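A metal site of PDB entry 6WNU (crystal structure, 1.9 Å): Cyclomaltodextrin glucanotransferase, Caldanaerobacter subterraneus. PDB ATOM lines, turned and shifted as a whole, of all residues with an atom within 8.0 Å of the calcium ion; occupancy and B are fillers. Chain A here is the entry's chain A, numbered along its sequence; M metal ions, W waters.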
ATOM      1  N   PRO A  54       5.034 -17.542 -22.102  1.00  0.00           N
ATOM      2  CA  PRO A  54       4.709 -17.777 -23.511  1.00  0.00           C
ATOM      3  C   PRO A  54       5.222 -19.124 -23.991  1.00  0.00           C
ATOM      4  O   PRO A  54       6.252 -19.623 -23.545  1.00  0.00           O
ATOM      5  CB  PRO A  54       5.431 -16.624 -24.227  1.00  0.00           C
ATOM      6  CG  PRO A  54       5.737 -15.605 -23.131  1.00  0.00           C
ATOM      7  CD  PRO A  54       6.011 -16.448 -21.946  1.00  0.00           C
ATOM      8  N   VAL A  56       6.652 -20.055 -26.705  1.00  0.00           N
ATOM      9  CA  VAL A  56       7.956 -20.057 -27.358  1.00  0.00           C
ATOM     10  C   VAL A  56       9.102 -20.069 -26.372  1.00  0.00           C
ATOM     11  O   VAL A  56      10.231 -20.432 -26.740  1.00  0.00           O
ATOM     12  CB  VAL A  56       8.035 -18.853 -28.310  1.00  0.00           C
ATOM     13  CG1 VAL A  56       8.435 -17.599 -27.538  1.00  0.00           C
ATOM     14  CG2 VAL A  56       8.988 -19.128 -29.443  1.00  0.00           C
ATOM     15  N   SER A  57       8.860 -19.681 -25.118  1.00  0.00           N
ATOM     16  CA  SER A  57       9.912 -19.549 -24.121  1.00  0.00           C
ATOM     17  C   SER A  57       9.381 -19.942 -22.749  1.00  0.00           C
ATOM     18  O   SER A  57       9.514 -19.215 -21.772  1.00  0.00           O
ATOM     19  CB  SER A  57      10.464 -18.132 -24.104  1.00  0.00           C
ATOM     20  OG  SER A  57       9.413 -17.162 -24.028  1.00  0.00           O
ATOM     21  N   MET A  60      10.091 -20.322 -17.619  1.00  0.00           N
ATOM     22  CA  MET A  60      10.953 -19.301 -17.031  1.00  0.00           C
ATOM     23  C   MET A  60      10.171 -18.276 -16.202  1.00  0.00           C
ATOM     24  O   MET A  60      10.680 -17.181 -15.943  1.00  0.00           O
ATOM     25  CB  MET A  60      11.757 -18.586 -18.125  1.00  0.00           C
ATOM     26  CG  MET A  60      12.798 -19.446 -18.809  1.00  0.00           C
ATOM     27  SD  MET A  60      13.968 -18.512 -19.805  1.00  0.00           S
ATOM     28  CE  MET A  60      12.958 -17.878 -21.126  1.00  0.00           C
ATOM     29  N   TYR A  71      11.539 -14.730 -14.738  1.00  0.00           N
ATOM     30  CA  TYR A  71      10.591 -13.672 -15.049  1.00  0.00           C
ATOM     31  C   TYR A  71       9.487 -13.667 -14.000  1.00  0.00           C
ATOM     32  O   TYR A  71       8.986 -14.734 -13.595  1.00  0.00           O
ATOM     33  CB  TYR A  71       9.954 -13.880 -16.410  1.00  0.00           C
ATOM     34  CG  TYR A  71      10.723 -13.550 -17.666  1.00  0.00           C
ATOM     35  CD1 TYR A  71      10.747 -12.253 -18.192  1.00  0.00           C
ATOM     36  CD2 TYR A  71      11.324 -14.565 -18.414  1.00  0.00           C
ATOM     37  CE1 TYR A  71      11.430 -11.973 -19.410  1.00  0.00           C
ATOM     38  CE2 TYR A  71      11.975 -14.293 -19.607  1.00  0.00           C
ATOM     39  CZ  TYR A  71      12.014 -13.016 -20.100  1.00  0.00           C
ATOM     40  OH  TYR A  71      12.659 -12.786 -21.294  1.00  0.00           O
ATOM     41  N   VAL A 100      14.233  -5.600 -26.340  1.00  0.00           N
ATOM     42  CA  VAL A 100      14.471  -6.497 -27.479  1.00  0.00           C
ATOM     43  C   VAL A 100      14.348  -7.953 -27.025  1.00  0.00           C
ATOM     44  O   VAL A 100      14.494  -8.289 -25.852  1.00  0.00           O
ATOM     45  CB  VAL A 100      15.842  -6.271 -28.146  1.00  0.00           C
ATOM     46  CG1 VAL A 100      15.999  -4.848 -28.620  1.00  0.00           C
ATOM     47  CG2 VAL A 100      16.981  -6.659 -27.210  1.00  0.00           C
ATOM     48  N   ASP A 101      14.090  -8.817 -27.998  1.00  0.00           N
ATOM     49  CA  ASP A 101      13.871 -10.228 -27.722  1.00  0.00           C
ATOM     50  C   ASP A 101      15.102 -10.845 -27.072  1.00  0.00           C
ATOM     51  O   ASP A 101      16.209 -10.781 -27.619  1.00  0.00           O
ATOM     52  CB  ASP A 101      13.527 -10.913 -29.041  1.00  0.00           C
ATOM     53  CG  ASP A 101      13.172 -12.373 -28.893  1.00  0.00           C
ATOM     54  OD1 ASP A 101      12.961 -12.870 -27.759  1.00  0.00           O
ATOM     55  OD2 ASP A 101      13.088 -13.034 -29.944  1.00  0.00           O
ATOM     56  N   ASN A 102      14.914 -11.422 -25.888  1.00  0.00           N
ATOM     57  CA  ASN A 102      15.936 -12.128 -25.136  1.00  0.00           C
ATOM     58  C   ASN A 102      15.772 -13.632 -25.285  1.00  0.00           C
ATOM     59  O   ASN A 102      14.745 -14.133 -25.744  1.00  0.00           O
ATOM     60  CB  ASN A 102      15.893 -11.726 -23.651  1.00  0.00           C
ATOM     61  CG  ASN A 102      16.739 -10.474 -23.343  1.00  0.00           C
ATOM     62  OD1 ASN A 102      17.472 -10.438 -22.330  1.00  0.00           O
ATOM     63  ND2 ASN A 102      16.648  -9.475 -24.189  1.00  0.00           N
ATOM     64  N   ILE A 103      16.802 -14.377 -24.842  1.00  0.00           N
ATOM     65  CA  ILE A 103      16.887 -15.801 -25.141  1.00  0.00           C
ATOM     66  C   ILE A 103      15.629 -16.534 -24.653  1.00  0.00           C
ATOM     67  O   ILE A 103      15.028 -16.202 -23.634  1.00  0.00           O
ATOM     68  CB  ILE A 103      18.144 -16.429 -24.538  1.00  0.00           C
ATOM     69  CG1 ILE A 103      18.191 -16.195 -23.021  1.00  0.00           C
ATOM     70  CG2 ILE A 103      19.400 -15.894 -25.263  1.00  0.00           C
ATOM     71  CD1 ILE A 103      19.339 -16.903 -22.314  1.00  0.00           C
ATOM     72  N   ASN A 104      15.272 -17.588 -25.386  1.00  0.00           N
ATOM     73  CA  ASN A 104      14.030 -18.301 -25.149  1.00  0.00           C
ATOM     74  C   ASN A 104      14.233 -19.591 -24.359  1.00  0.00           C
ATOM     75  O   ASN A 104      13.244 -20.231 -24.016  1.00  0.00           O
ATOM     76  CB  ASN A 104      13.339 -18.583 -26.492  1.00  0.00           C
ATOM     77  CG  ASN A 104      12.852 -17.317 -27.147  1.00  0.00           C
ATOM     78  OD1 ASN A 104      12.750 -16.278 -26.498  1.00  0.00           O
ATOM     79  ND2 ASN A 104      12.552 -17.392 -28.438  1.00  0.00           N
ATOM     80  N   LYS A 105      15.479 -19.956 -24.064  1.00  0.00           N
ATOM     81  CA  LYS A 105      15.914 -20.976 -23.114  1.00  0.00           C
ATOM     82  C   LYS A 105      16.703 -20.281 -22.002  1.00  0.00           C
ATOM     83  O   LYS A 105      17.416 -19.323 -22.282  1.00  0.00           O
ATOM     84  CB  LYS A 105      16.837 -22.037 -23.741  1.00  0.00           C
ATOM     85  CG  LYS A 105      16.234 -23.000 -24.732  1.00  0.00           C
ATOM     86  CD  LYS A 105      17.344 -23.959 -25.258  1.00  0.00           C
ATOM     87  CE  LYS A 105      17.926 -24.899 -24.152  1.00  0.00           C
ATOM     88  NZ  LYS A 105      19.305 -24.551 -23.573  1.00  0.00           N
ATOM     89  N   PRO A 116      16.500 -14.541 -18.624  1.00  0.00           N
ATOM     90  CA  PRO A 116      16.915 -13.186 -19.006  1.00  0.00           C
ATOM     91  C   PRO A 116      15.862 -12.143 -18.647  1.00  0.00           C
ATOM     92  O   PRO A 116      15.489 -11.313 -19.464  1.00  0.00           O
ATOM     93  CB  PRO A 116      17.074 -13.296 -20.529  1.00  0.00           C
ATOM     94  CG  PRO A 116      15.986 -14.295 -20.902  1.00  0.00           C
ATOM     95  CD  PRO A 116      16.005 -15.317 -19.784  1.00  0.00           C
ATOM     96  N   TRP A 121      20.207 -10.014 -22.194  1.00  0.00           N
ATOM     97  CA  TRP A 121      20.691 -11.187 -22.912  1.00  0.00           C
ATOM     98  C   TRP A 121      19.899 -11.318 -24.221  1.00  0.00           C
ATOM     99  O   TRP A 121      19.044 -12.184 -24.362  1.00  0.00           O
ATOM    100  CB  TRP A 121      20.582 -12.433 -22.044  1.00  0.00           C
ATOM    101  CG  TRP A 121      21.396 -12.407 -20.792  1.00  0.00           C
ATOM    102  CD1 TRP A 121      22.370 -11.510 -20.452  1.00  0.00           C
ATOM    103  CD2 TRP A 121      21.288 -13.311 -19.682  1.00  0.00           C
ATOM    104  NE1 TRP A 121      22.872 -11.810 -19.217  1.00  0.00           N
ATOM    105  CE2 TRP A 121      22.221 -12.904 -18.715  1.00  0.00           C
ATOM    106  CE3 TRP A 121      20.475 -14.421 -19.410  1.00  0.00           C
ATOM    107  CZ2 TRP A 121      22.374 -13.568 -17.506  1.00  0.00           C
ATOM    108  CZ3 TRP A 121      20.637 -15.072 -18.216  1.00  0.00           C
ATOM    109  CH2 TRP A 121      21.579 -14.652 -17.278  1.00  0.00           C
ATOM    110  N   ALA A 122      20.207 -10.446 -25.174  1.00  0.00           N
ATOM    111  CA  ALA A 122      19.476 -10.384 -26.432  1.00  0.00           C
ATOM    112  C   ALA A 122      19.685 -11.634 -27.275  1.00  0.00           C
ATOM    113  O   ALA A 122      20.797 -12.173 -27.363  1.00  0.00           O
ATOM    114  CB  ALA A 122      19.910  -9.160 -27.236  1.00  0.00           C
ATOM    115  N   ARG A 123      18.594 -12.105 -27.904  1.00  0.00           N
ATOM    116  CA  ARG A 123      18.691 -13.021 -29.040  1.00  0.00           C
ATOM    117  C   ARG A 123      18.372 -12.360 -30.376  1.00  0.00           C
ATOM    118  O   ARG A 123      18.876 -12.834 -31.410  1.00  0.00           O
ATOM    119  CB  ARG A 123      17.759 -14.232 -28.842  1.00  0.00           C
ATOM    120  CG  ARG A 123      16.386 -14.074 -29.471  1.00  0.00           C
ATOM    121  CD  ARG A 123      15.386 -15.113 -28.994  1.00  0.00           C
ATOM    122  NE  ARG A 123      15.662 -16.506 -29.345  1.00  0.00           N
ATOM    123  CZ  ARG A 123      15.256 -17.093 -30.473  1.00  0.00           C
ATOM    124  NH1 ARG A 123      14.596 -16.398 -31.372  1.00  0.00           N
ATOM    125  NH2 ARG A 123      15.529 -18.372 -30.712  1.00  0.00           N
ATOM    126  N   ASP A 124      17.592 -11.278 -30.401  1.00  0.00           N
ATOM    127  CA  ASP A 124      17.116 -10.695 -31.657  1.00  0.00           C
ATOM    128  C   ASP A 124      16.849  -9.222 -31.397  1.00  0.00           C
ATOM    129  O   ASP A 124      15.885  -8.878 -30.716  1.00  0.00           O
ATOM    130  CB  ASP A 124      15.857 -11.402 -32.160  1.00  0.00           C
ATOM    131  CG  ASP A 124      15.497 -11.060 -33.597  1.00  0.00           C
ATOM    132  OD1 ASP A 124      15.820  -9.951 -34.078  1.00  0.00           O
ATOM    133  OD2 ASP A 124      14.849 -11.900 -34.263  1.00  0.00           O
ATOM    134  N   ARG A 127      13.232  -7.568 -32.680  1.00  0.00           N
ATOM    135  CA  ARG A 127      11.922  -7.993 -32.215  1.00  0.00           C
ATOM    136  C   ARG A 127      11.722  -7.590 -30.760  1.00  0.00           C
ATOM    137  O   ARG A 127      12.691  -7.447 -30.015  1.00  0.00           O
ATOM    138  CB  ARG A 127      11.728  -9.515 -32.340  1.00  0.00           C
ATOM    139  CG  ARG A 127      11.641 -10.028 -33.770  1.00  0.00           C
ATOM    140  CD  ARG A 127      11.416 -11.526 -33.747  1.00  0.00           C
ATOM    141  NE  ARG A 127      10.801 -12.005 -34.972  1.00  0.00           N
ATOM    142  CZ  ARG A 127      10.608 -13.280 -35.272  1.00  0.00           C
ATOM    143  NH1 ARG A 127      11.009 -14.229 -34.422  1.00  0.00           N
ATOM    144  NH2 ARG A 127      10.053 -13.620 -36.421  1.00  0.00           N
ATOM    145  N   VAL A 128      10.455  -7.420 -30.361  1.00  0.00           N
ATOM    146  CA  VAL A 128      10.115  -7.143 -28.964  1.00  0.00           C
ATOM    147  C   VAL A 128      10.088  -8.458 -28.188  1.00  0.00           C
ATOM    148  O   VAL A 128       9.659  -9.489 -28.704  1.00  0.00           O
ATOM    149  CB  VAL A 128       8.775  -6.406 -28.853  1.00  0.00           C
ATOM    150  CG1 VAL A 128       8.549  -5.946 -27.406  1.00  0.00           C
ATOM    151  CG2 VAL A 128       8.729  -5.217 -29.789  1.00  0.00           C
ATOM    152  N   GLU A 129      10.546  -8.399 -26.946  1.00  0.00           N
ATOM    153  CA  GLU A 129      10.491  -9.553 -26.066  1.00  0.00           C
ATOM    154  C   GLU A 129       9.034  -9.962 -25.824  1.00  0.00           C
ATOM    155  O   GLU A 129       8.221  -9.143 -25.371  1.00  0.00           O
ATOM    156  CB  GLU A 129      11.201  -9.235 -24.753  1.00  0.00           C
ATOM    157  CG  GLU A 129      11.069 -10.285 -23.667  1.00  0.00           C
ATOM    158  CD  GLU A 129      11.354 -11.697 -24.156  1.00  0.00           C
ATOM    159  OE1 GLU A 129      12.456 -11.953 -24.687  1.00  0.00           O
ATOM    160  OE2 GLU A 129      10.472 -12.569 -23.986  1.00  0.00           O
ATOM    161  N   GLU A 130       8.721 -11.233 -26.087  1.00  0.00           N
ATOM    162  CA  GLU A 130       7.344 -11.706 -26.015  1.00  0.00           C
ATOM    163  C   GLU A 130       6.807 -11.788 -24.579  1.00  0.00           C
ATOM    164  O   GLU A 130       5.589 -11.737 -24.398  1.00  0.00           O
ATOM    165  CB  GLU A 130       7.240 -13.058 -26.736  1.00  0.00           C
ATOM    166  CG  GLU A 130       7.926 -14.215 -26.046  1.00  0.00           C
ATOM    167  CD  GLU A 130       9.452 -14.236 -26.215  1.00  0.00           C
ATOM    168  OE1 GLU A 130      10.005 -13.402 -26.950  1.00  0.00           O
ATOM    169  OE2 GLU A 130      10.079 -15.123 -25.612  1.00  0.00           O
ATOM    170  N   HIS A 131       7.674 -11.949 -23.570  1.00  0.00           N
ATOM    171  CA  HIS A 131       7.199 -11.800 -22.190  1.00  0.00           C
ATOM    172  C   HIS A 131       6.665 -10.402 -21.919  1.00  0.00           C
ATOM    173  O   HIS A 131       5.769 -10.229 -21.083  1.00  0.00           O
ATOM    174  CB  HIS A 131       8.309 -12.108 -21.168  1.00  0.00           C
ATOM    175  CG  HIS A 131       8.604 -13.573 -20.997  1.00  0.00           C
ATOM    176  ND1 HIS A 131       9.300 -14.312 -21.931  1.00  0.00           N
ATOM    177  CD2 HIS A 131       8.307 -14.427 -19.981  1.00  0.00           C
ATOM    178  CE1 HIS A 131       9.412 -15.554 -21.505  1.00  0.00           C
ATOM    179  NE2 HIS A 131       8.825 -15.649 -20.328  1.00  0.00           N
ATOM    180  N   PHE A 132       7.184  -9.392 -22.629  1.00  0.00           N
ATOM    181  CA  PHE A 132       6.831  -7.998 -22.375  1.00  0.00           C
ATOM    182  C   PHE A 132       5.724  -7.485 -23.260  1.00  0.00           C
ATOM    183  O   PHE A 132       4.989  -6.576 -22.841  1.00  0.00           O
ATOM    184  CB  PHE A 132       8.064  -7.079 -22.510  1.00  0.00           C
ATOM    185  CG  PHE A 132       9.175  -7.393 -21.553  1.00  0.00           C
ATOM    186  CD1 PHE A 132       8.925  -8.154 -20.404  1.00  0.00           C
ATOM    187  CD2 PHE A 132      10.478  -6.943 -21.788  1.00  0.00           C
ATOM    188  CE1 PHE A 132       9.941  -8.462 -19.506  1.00  0.00           C
ATOM    189  CE2 PHE A 132      11.501  -7.250 -20.884  1.00  0.00           C
ATOM    190  CZ  PHE A 132      11.235  -8.004 -19.746  1.00  0.00           C
ATOM    191  N   GLU A 173      21.152 -20.358 -25.112  1.00  0.00           N
ATOM    192  CA  GLU A 173      21.001 -20.434 -26.559  1.00  0.00           C
ATOM    193  C   GLU A 173      22.336 -20.242 -27.273  1.00  0.00           C
ATOM    194  O   GLU A 173      22.358 -19.782 -28.419  1.00  0.00           O
ATOM    195  CB  GLU A 173      19.986 -19.416 -27.070  1.00  0.00           C
ATOM    196  CG  GLU A 173      18.540 -19.810 -26.715  1.00  0.00           C
ATOM    197  CD  GLU A 173      17.500 -19.238 -27.663  1.00  0.00           C
ATOM    198  OE1 GLU A 173      17.138 -18.042 -27.523  1.00  0.00           O
ATOM    199  OE2 GLU A 173      17.038 -19.984 -28.562  1.00  0.00           O
HETATM  200 CA    CA M   1      12.283 -14.034 -25.851  1.00  0.00          CA
HETATM  201  O   HOH W   1      12.658 -14.758 -23.553  1.00  0.00           O
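The calcium ion is bound by the side-chain carboxylate (OD1) of Asp 101 (2.3 Å). OD1 of Asn 104 is bound to the calcium ion (2.4 Å). OE1 of Glu 129 is bound to the calcium ion (2.4 Å). Water W1 is bound to the calcium ion. O of Asn 102 is bound to the calcium ion (2.5 Å). OE2 of Glu 130 binds the calcium ion, at 2.5 Å. The calcium ion is bound by OE1 of Glu 130 (2.6 Å). The calcium ion has seven donor atoms within binding distance. Slightly farther from the calcium ion lies OE2 of Glu 129 (3.0 Å).
The guanidinium group of Arg 123 lies within salt-bridge range of the side-chain carboxylate of Asp 101 (3.95 Å). The backbone NH of Asp 124 sits at hydrogen-bond distance from the backbone carbonyl oxygen of Asp 101 (3.1 Å). The backbone NH (N) of Asp 101 is in hydrogen-bond range of the backbone carbonyl oxygen (O) of Arg 127 (2.8 Å). ND2 of Asn 104 lies close to NE of Arg 123. The side-chain carboxylate of Glu 173 lies within hydrogen-bond range of the backbone NH of Asn 104, at 2.9 Å. The backbone NH (N) of His 131 lies within hydrogen-bond range of the side-chain carboxylate (OE2) of Glu 129, at 2.9 Å. The backbone carbonyl oxygen (O) of Val 100 sits at hydrogen-bond distance from the side-chain amide nitrogen (ND2) of Asn 102, at 3.0 Å. The side-chain carboxylate (OE2) of Glu 130 sits close to the side-chain hydroxyl (OG) of Ser 57.
Water W1 lies within hydrogen-bond range of the backbone carbonyl oxygen of Ile 103 (2.8 Å), the side-chain hydroxyl of Tyr 71 (3.0 Å) and the side-chain carboxylate of Glu 129 (3.1 Å).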
